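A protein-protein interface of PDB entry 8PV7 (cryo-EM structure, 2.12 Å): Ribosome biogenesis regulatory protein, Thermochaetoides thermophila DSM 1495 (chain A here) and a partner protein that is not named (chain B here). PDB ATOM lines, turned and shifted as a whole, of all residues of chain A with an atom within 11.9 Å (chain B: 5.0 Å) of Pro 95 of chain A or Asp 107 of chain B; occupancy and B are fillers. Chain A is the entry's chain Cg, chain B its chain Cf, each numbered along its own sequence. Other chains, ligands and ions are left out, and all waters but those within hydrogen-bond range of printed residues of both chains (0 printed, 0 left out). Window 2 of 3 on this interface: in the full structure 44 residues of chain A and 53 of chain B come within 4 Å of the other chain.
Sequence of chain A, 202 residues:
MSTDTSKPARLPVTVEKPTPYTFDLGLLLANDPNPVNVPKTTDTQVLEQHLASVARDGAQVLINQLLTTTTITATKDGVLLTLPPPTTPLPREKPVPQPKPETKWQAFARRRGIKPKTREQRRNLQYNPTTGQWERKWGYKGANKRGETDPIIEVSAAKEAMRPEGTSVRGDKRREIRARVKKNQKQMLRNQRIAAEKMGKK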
ATOM      1  N   LEU A  90      -6.873  -3.184  -2.024  1.00  0.00           N
ATOM      2  CA  LEU A  90      -7.123  -3.106  -3.452  1.00  0.00           C
ATOM      3  C   LEU A  90      -8.407  -3.857  -3.756  1.00  0.00           C
ATOM      4  O   LEU A  90      -8.711  -4.859  -3.098  1.00  0.00           O
ATOM      5  CB  LEU A  90      -5.963  -3.705  -4.263  1.00  0.00           C
ATOM      6  CG  LEU A  90      -4.654  -2.915  -4.260  1.00  0.00           C
ATOM      7  CD1 LEU A  90      -3.510  -3.786  -4.735  1.00  0.00           C
ATOM      8  CD2 LEU A  90      -4.772  -1.673  -5.124  1.00  0.00           C
ATOM      9  N   PRO A  91      -9.191  -3.389  -4.725  1.00  0.00           N
ATOM     10  CA  PRO A  91     -10.448  -4.073  -5.039  1.00  0.00           C
ATOM     11  C   PRO A  91     -10.218  -5.419  -5.704  1.00  0.00           C
ATOM     12  O   PRO A  91      -9.244  -5.622  -6.430  1.00  0.00           O
ATOM     13  CB  PRO A  91     -11.151  -3.098  -5.988  1.00  0.00           C
ATOM     14  CG  PRO A  91     -10.055  -2.323  -6.596  1.00  0.00           C
ATOM     15  CD  PRO A  91      -9.012  -2.174  -5.536  1.00  0.00           C
ATOM     16  N   ARG A  92     -11.135  -6.342  -5.444  1.00  0.00           N
ATOM     17  CA  ARG A  92     -11.160  -7.606  -6.153  1.00  0.00           C
ATOM     18  C   ARG A  92     -11.731  -7.401  -7.550  1.00  0.00           C
ATOM     19  O   ARG A  92     -12.357  -6.382  -7.850  1.00  0.00           O
ATOM     20  CB  ARG A  92     -11.998  -8.630  -5.392  1.00  0.00           C
ATOM     21  CG  ARG A  92     -11.322  -9.203  -4.172  1.00  0.00           C
ATOM     22  CD  ARG A  92     -12.290 -10.020  -3.342  1.00  0.00           C
ATOM     23  NE  ARG A  92     -12.908 -11.090  -4.113  1.00  0.00           N
ATOM     24  CZ  ARG A  92     -12.462 -12.337  -4.153  1.00  0.00           C
ATOM     25  NH1 ARG A  92     -11.391 -12.709  -3.476  1.00  0.00           N
ATOM     26  NH2 ARG A  92     -13.106 -13.233  -4.894  1.00  0.00           N
ATOM     27  N   GLU A  93     -11.494  -8.378  -8.418  1.00  0.00           N
ATOM     28  CA  GLU A  93     -12.105  -8.351  -9.738  1.00  0.00           C
ATOM     29  C   GLU A  93     -13.464  -9.025  -9.756  1.00  0.00           C
ATOM     30  O   GLU A  93     -14.348  -8.609 -10.511  1.00  0.00           O
ATOM     31  CB  GLU A  93     -11.189  -9.017 -10.766  1.00  0.00           C
ATOM     32  CG  GLU A  93     -10.411 -10.203 -10.241  1.00  0.00           C
ATOM     33  CD  GLU A  93      -9.912 -11.105 -11.351  1.00  0.00           C
ATOM     34  OE1 GLU A  93      -8.984 -11.902 -11.100  1.00  0.00           O
ATOM     35  OE2 GLU A  93     -10.441 -11.014 -12.477  1.00  0.00           O
ATOM     36  N   LYS A  94     -13.651 -10.049  -8.934  1.00  0.00           N
ATOM     37  CA  LYS A  94     -14.882 -10.810  -8.853  1.00  0.00           C
ATOM     38  C   LYS A  94     -15.304 -10.933  -7.399  1.00  0.00           C
ATOM     39  O   LYS A  94     -14.462 -10.855  -6.499  1.00  0.00           O
ATOM     40  CB  LYS A  94     -14.699 -12.203  -9.474  1.00  0.00           C
ATOM     41  CG  LYS A  94     -14.491 -12.156 -10.972  1.00  0.00           C
ATOM     42  CD  LYS A  94     -13.925 -13.448 -11.510  1.00  0.00           C
ATOM     43  CE  LYS A  94     -13.524 -13.282 -12.964  1.00  0.00           C
ATOM     44  NZ  LYS A  94     -12.818 -14.477 -13.486  1.00  0.00           N
ATOM     45  N   PRO A  95     -16.602 -11.092  -7.137  1.00  0.00           N
ATOM     46  CA  PRO A  95     -17.058 -11.233  -5.751  1.00  0.00           C
ATOM     47  C   PRO A  95     -16.565 -12.524  -5.120  1.00  0.00           C
ATOM     48  O   PRO A  95     -16.208 -13.482  -5.809  1.00  0.00           O
ATOM     49  CB  PRO A  95     -18.586 -11.219  -5.873  1.00  0.00           C
ATOM     50  CG  PRO A  95     -18.868 -11.508  -7.297  1.00  0.00           C
ATOM     51  CD  PRO A  95     -17.734 -10.935  -8.063  1.00  0.00           C
ATOM     52  N   VAL A  96     -16.516 -12.516  -3.791  1.00  0.00           N
ATOM     53  CA  VAL A  96     -16.089 -13.689  -3.020  1.00  0.00           C
ATOM     54  C   VAL A  96     -17.063 -14.831  -3.272  1.00  0.00           C
ATOM     55  O   VAL A  96     -18.288 -14.596  -3.304  1.00  0.00           O
ATOM     56  CB  VAL A  96     -16.012 -13.342  -1.523  1.00  0.00           C
ATOM     57  CG1 VAL A  96     -15.818 -14.581  -0.671  1.00  0.00           C
ATOM     58  CG2 VAL A  96     -14.895 -12.349  -1.273  1.00  0.00           C
ATOM     59  N   PRO A  97     -16.591 -16.055  -3.520  1.00  0.00           N
ATOM     60  CA  PRO A  97     -17.508 -17.177  -3.753  1.00  0.00           C
ATOM     61  C   PRO A  97     -18.399 -17.444  -2.550  1.00  0.00           C
ATOM     62  O   PRO A  97     -17.972 -17.337  -1.399  1.00  0.00           O
ATOM     63  CB  PRO A  97     -16.564 -18.352  -4.021  1.00  0.00           C
ATOM     64  CG  PRO A  97     -15.315 -17.731  -4.490  1.00  0.00           C
ATOM     65  CD  PRO A  97     -15.189 -16.437  -3.758  1.00  0.00           C
ATOM     66  N   GLN A  98     -19.643 -17.798  -2.832  1.00  0.00           N
ATOM     67  CA  GLN A  98     -20.664 -18.059  -1.837  1.00  0.00           C
ATOM     68  C   GLN A  98     -21.151 -19.493  -1.981  1.00  0.00           C
ATOM     69  O   GLN A  98     -20.996 -20.102  -3.046  1.00  0.00           O
ATOM     70  CB  GLN A  98     -21.842 -17.083  -2.000  1.00  0.00           C
ATOM     71  CG  GLN A  98     -21.580 -15.628  -1.573  1.00  0.00           C
ATOM     72  CD  GLN A  98     -21.002 -15.440  -0.166  1.00  0.00           C
ATOM     73  OE1 GLN A  98     -21.133 -16.296   0.711  1.00  0.00           O
ATOM     74  NE2 GLN A  98     -20.351 -14.304   0.042  1.00  0.00           N
ATOM     75  N   PRO A  99     -21.696 -20.082  -0.915  1.00  0.00           N
ATOM     76  CA  PRO A  99     -22.301 -21.413  -1.041  1.00  0.00           C
ATOM     77  C   PRO A  99     -23.472 -21.413  -2.014  1.00  0.00           C
ATOM     78  O   PRO A  99     -24.263 -20.469  -2.067  1.00  0.00           O
ATOM     79  CB  PRO A  99     -22.758 -21.728   0.385  1.00  0.00           C
ATOM     80  CG  PRO A  99     -21.855 -20.929   1.247  1.00  0.00           C
ATOM     81  CD  PRO A  99     -21.585 -19.664   0.494  1.00  0.00           C
ATOM     82  N   PRO B  21     -15.201 -17.301 -10.026  1.00  0.00           N
ATOM     83  CA  PRO B  21     -14.718 -16.572  -8.845  1.00  0.00           C
ATOM     84  C   PRO B  21     -14.017 -17.487  -7.853  1.00  0.00           C
ATOM     85  O   PRO B  21     -14.434 -18.624  -7.624  1.00  0.00           O
ATOM     86  CB  PRO B  21     -16.001 -15.981  -8.251  1.00  0.00           C
ATOM     87  CG  PRO B  21     -16.931 -15.886  -9.400  1.00  0.00           C
ATOM     88  CD  PRO B  21     -16.638 -17.082 -10.252  1.00  0.00           C
ATOM     89  N   LYS B  22     -12.948 -16.972  -7.248  1.00  0.00           N
ATOM     90  CA  LYS B  22     -12.096 -17.756  -6.368  1.00  0.00           C
ATOM     91  C   LYS B  22     -11.805 -16.973  -5.099  1.00  0.00           C
ATOM     92  O   LYS B  22     -11.901 -15.745  -5.065  1.00  0.00           O
ATOM     93  CB  LYS B  22     -10.773 -18.143  -7.046  1.00  0.00           C
ATOM     94  CG  LYS B  22     -10.931 -19.014  -8.274  1.00  0.00           C
ATOM     95  CD  LYS B  22      -9.651 -19.085  -9.080  1.00  0.00           C
ATOM     96  CE  LYS B  22      -9.852 -19.916 -10.333  1.00  0.00           C
ATOM     97  NZ  LYS B  22      -8.635 -19.948 -11.181  1.00  0.00           N
ATOM     98  N   GLU B  25      -7.699 -14.902  -5.906  1.00  0.00           N
ATOM     99  CA  GLU B  25      -7.986 -14.541  -7.281  1.00  0.00           C
ATOM    100  C   GLU B  25      -6.751 -14.688  -8.166  1.00  0.00           C
ATOM    101  O   GLU B  25      -5.610 -14.684  -7.699  1.00  0.00           O
ATOM    102  CB  GLU B  25      -8.505 -13.108  -7.353  1.00  0.00           C
ATOM    103  CG  GLU B  25      -9.917 -12.947  -6.836  1.00  0.00           C
ATOM    104  CD  GLU B  25     -10.431 -11.537  -6.995  1.00  0.00           C
ATOM    105  OE1 GLU B  25      -9.617 -10.593  -6.910  1.00  0.00           O
ATOM    106  OE2 GLU B  25     -11.644 -11.371  -7.224  1.00  0.00           O
ATOM    107  N   MET B 105     -12.755  -2.825 -13.444  1.00  0.00           N
ATOM    108  CA  MET B 105     -14.007  -3.557 -13.478  1.00  0.00           C
ATOM    109  C   MET B 105     -14.175  -4.375 -12.206  1.00  0.00           C
ATOM    110  O   MET B 105     -13.198  -4.749 -11.554  1.00  0.00           O
ATOM    111  CB  MET B 105     -14.054  -4.508 -14.681  1.00  0.00           C
ATOM    112  CG  MET B 105     -13.872  -3.841 -16.024  1.00  0.00           C
ATOM    113  SD  MET B 105     -15.015  -2.487 -16.289  1.00  0.00           S
ATOM    114  CE  MET B 105     -16.246  -3.304 -17.288  1.00  0.00           C
ATOM    115  N   PHE B 106     -15.428  -4.650 -11.861  1.00  0.00           N
ATOM    116  CA  PHE B 106     -15.759  -5.594 -10.804  1.00  0.00           C
ATOM    117  C   PHE B 106     -16.983  -6.376 -11.240  1.00  0.00           C
ATOM    118  O   PHE B 106     -18.013  -5.774 -11.552  1.00  0.00           O
ATOM    119  CB  PHE B 106     -16.027  -4.891  -9.469  1.00  0.00           C
ATOM    120  CG  PHE B 106     -16.436  -5.826  -8.367  1.00  0.00           C
ATOM    121  CD1 PHE B 106     -15.519  -6.695  -7.800  1.00  0.00           C
ATOM    122  CD2 PHE B 106     -17.740  -5.842  -7.902  1.00  0.00           C
ATOM    123  CE1 PHE B 106     -15.891  -7.557  -6.792  1.00  0.00           C
ATOM    124  CE2 PHE B 106     -18.117  -6.703  -6.890  1.00  0.00           C
ATOM    125  CZ  PHE B 106     -17.191  -7.561  -6.335  1.00  0.00           C
ATOM    126  N   ASP B 107     -16.858  -7.705 -11.260  1.00  0.00           N
ATOM    127  CA  ASP B 107     -17.923  -8.616 -11.697  1.00  0.00           C
ATOM    128  C   ASP B 107     -18.423  -8.264 -13.096  1.00  0.00           C
ATOM    129  O   ASP B 107     -19.627  -8.253 -13.361  1.00  0.00           O
ATOM    130  CB  ASP B 107     -19.077  -8.641 -10.692  1.00  0.00           C
ATOM    131  CG  ASP B 107     -19.839  -9.947 -10.712  1.00  0.00           C
ATOM    132  OD1 ASP B 107     -19.384 -10.893 -11.389  1.00  0.00           O
ATOM    133  OD2 ASP B 107     -20.895 -10.029 -10.052  1.00  0.00           O
ATOM    134  N   TYR B 108     -17.475  -7.946 -13.986  1.00  0.00           N
ATOM    135  CA  TYR B 108     -17.723  -7.567 -15.383  1.00  0.00           C
ATOM    136  C   TYR B 108     -18.601  -6.324 -15.501  1.00  0.00           C
ATOM    137  O   TYR B 108     -19.308  -6.142 -16.492  1.00  0.00           O
ATOM    138  CB  TYR B 108     -18.326  -8.724 -16.187  1.00  0.00           C
ATOM    139  CG  TYR B 108     -17.606 -10.034 -15.995  1.00  0.00           C
ATOM    140  CD1 TYR B 108     -16.246 -10.145 -16.247  1.00  0.00           C
ATOM    141  CD2 TYR B 108     -18.287 -11.161 -15.562  1.00  0.00           C
ATOM    142  CE1 TYR B 108     -15.585 -11.345 -16.072  1.00  0.00           C
ATOM    143  CE2 TYR B 108     -17.637 -12.361 -15.386  1.00  0.00           C
ATOM    144  CZ  TYR B 108     -16.289 -12.448 -15.642  1.00  0.00           C
ATOM    145  OH  TYR B 108     -15.646 -13.647 -15.466  1.00  0.00           O
ATOM    146  N   LYS B 109     -18.545  -5.453 -14.498  1.00  0.00           N
ATOM    147  CA  LYS B 109     -19.240  -4.177 -14.519  1.00  0.00           C
ATOM    148  C   LYS B 109     -18.251  -3.100 -14.114  1.00  0.00           C
ATOM    149  O   LYS B 109     -17.272  -3.376 -13.420  1.00  0.00           O
ATOM    150  CB  LYS B 109     -20.449  -4.170 -13.581  1.00  0.00           C
ATOM    151  CG  LYS B 109     -21.706  -4.754 -14.190  1.00  0.00           C
ATOM    152  CD  LYS B 109     -22.819  -4.858 -13.166  1.00  0.00           C
ATOM    153  CE  LYS B 109     -22.646  -6.082 -12.285  1.00  0.00           C
ATOM    154  NZ  LYS B 109     -21.943  -5.763 -11.011  1.00  0.00           N
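The side-chain carboxylate of Glu 25 of chain B is in hydrogen-bond range of the backbone NH of Lys 94 of chain A (2.9 Å). The backbone carbonyl oxygen (O) of Lys 22 of chain B lies within hydrogen-bond range of the guanidinium group (NH2) of Arg 92 of chain A. The backbone NH (N) of Asp 107 of chain B sits at hydrogen-bond distance from the backbone carbonyl oxygen (O) of Glu 93 of chain A, 2.8 Å away. OE2 of Glu 25 of chain B lies within salt-bridge range of NH2 of Arg 92 of chain A, 3.3 Å away. The backbone NH (N) of Glu 93 of chain A is in hydrogen-bond range of the side-chain carboxylate (OE2) of Glu 25 of chain B, at 3.2 Å.
The guanidinium group (NE) of Arg 92 of chain A sits at hydrogen-bond distance from the backbone carbonyl oxygen (O) of Lys 94 of chain A. O of Pro 95 of chain A sits at hydrogen-bond distance from NH2 of Arg 92 of chain A.
Among the printed residues, merely in contact across the chains: Arg 92 of chain A with Phe 106 of chain B (3.2 Å), Lys 94 of chain A with Tyr 108 of chain B (3.3 Å), Glu 93 of chain A with Phe 106 of chain B (3.3 Å), Pro 97 of chain A with Pro 21 of chain B (3.4 Å), Lys 94 of chain A with Phe 106 of chain B (3.5 Å), Pro 95 of chain A with Pro 21 of chain B (3.5 Å), Pro 95 of chain A with Asp 107 of chain B (3.5 Å), Pro 97 of chain A with Lys 22 of chain B (3.6 Å) and Pro 95 of chain A with Phe 106 of chain B (3.6 Å).
Pro 91 of chain A touches none of the printed residues of chain B. Of the printed residues of chain B, Arg 92 of chain A touches Lys 22, Glu 25 and Phe 106. Of the printed residues of chain B, Lys 94 of chain A touches Glu 25 (2.9 Å), Phe 106 (3.5 Å) and Tyr 108 (3.3 Å). Pro 95 of chain A touches just these residues of chain B: Pro 21 (3.5 Å), Phe 106 (3.6 Å) and Asp 107 (3.5 Å). Of the printed residues of chain B, Pro 97 of chain A touches Pro 21 (3.4 Å) and Lys 22 (3.6 Å). Pro 99 of chain A touches none of the printed residues of chain B. Of the printed residues of chain A, Lys 22 of chain B touches Arg 92 (2.8 Å) and Pro 97 (3.6 Å). Of the printed residues of chain A, Glu 25 of chain B touches Arg 92, Glu 93 and Lys 94. No residue of chain A comes within 4 Å of Met 105 of chain B. Of chain A, only Glu 93 and Pro 95 come within 4 Å of Asp 107 of chain B. Tyr 108 of chain B touches just one residue of chain A: Lys 94 (3.3 Å). Lys 109 of chain B touches none of the printed residues of chain A. The nearest printed residue of chain B that does not touch Pro 97 of chain A is Glu 25 of chain B (7.0 Å).
Of the 10 printed residues of chain A, 5 touch a printed residue of chain B. Printed residues of chain A that touch a printed residue of chain B: Arg 92, Glu 93, Lys 94, Pro 95 and Pro 97. Hydrophobic or aromatic side chains of chain A that line the printed part of chain B: Pro 95 and Pro 97. Of the 8 printed residues of chain B, 6 touch a printed residue of chain A. Among the printed residues, Asp or Glu carboxylates within 4 Å of a Lys or Arg side-chain nitrogen of the other chain: Arg 92 of chain A with Glu 25 of chain B.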
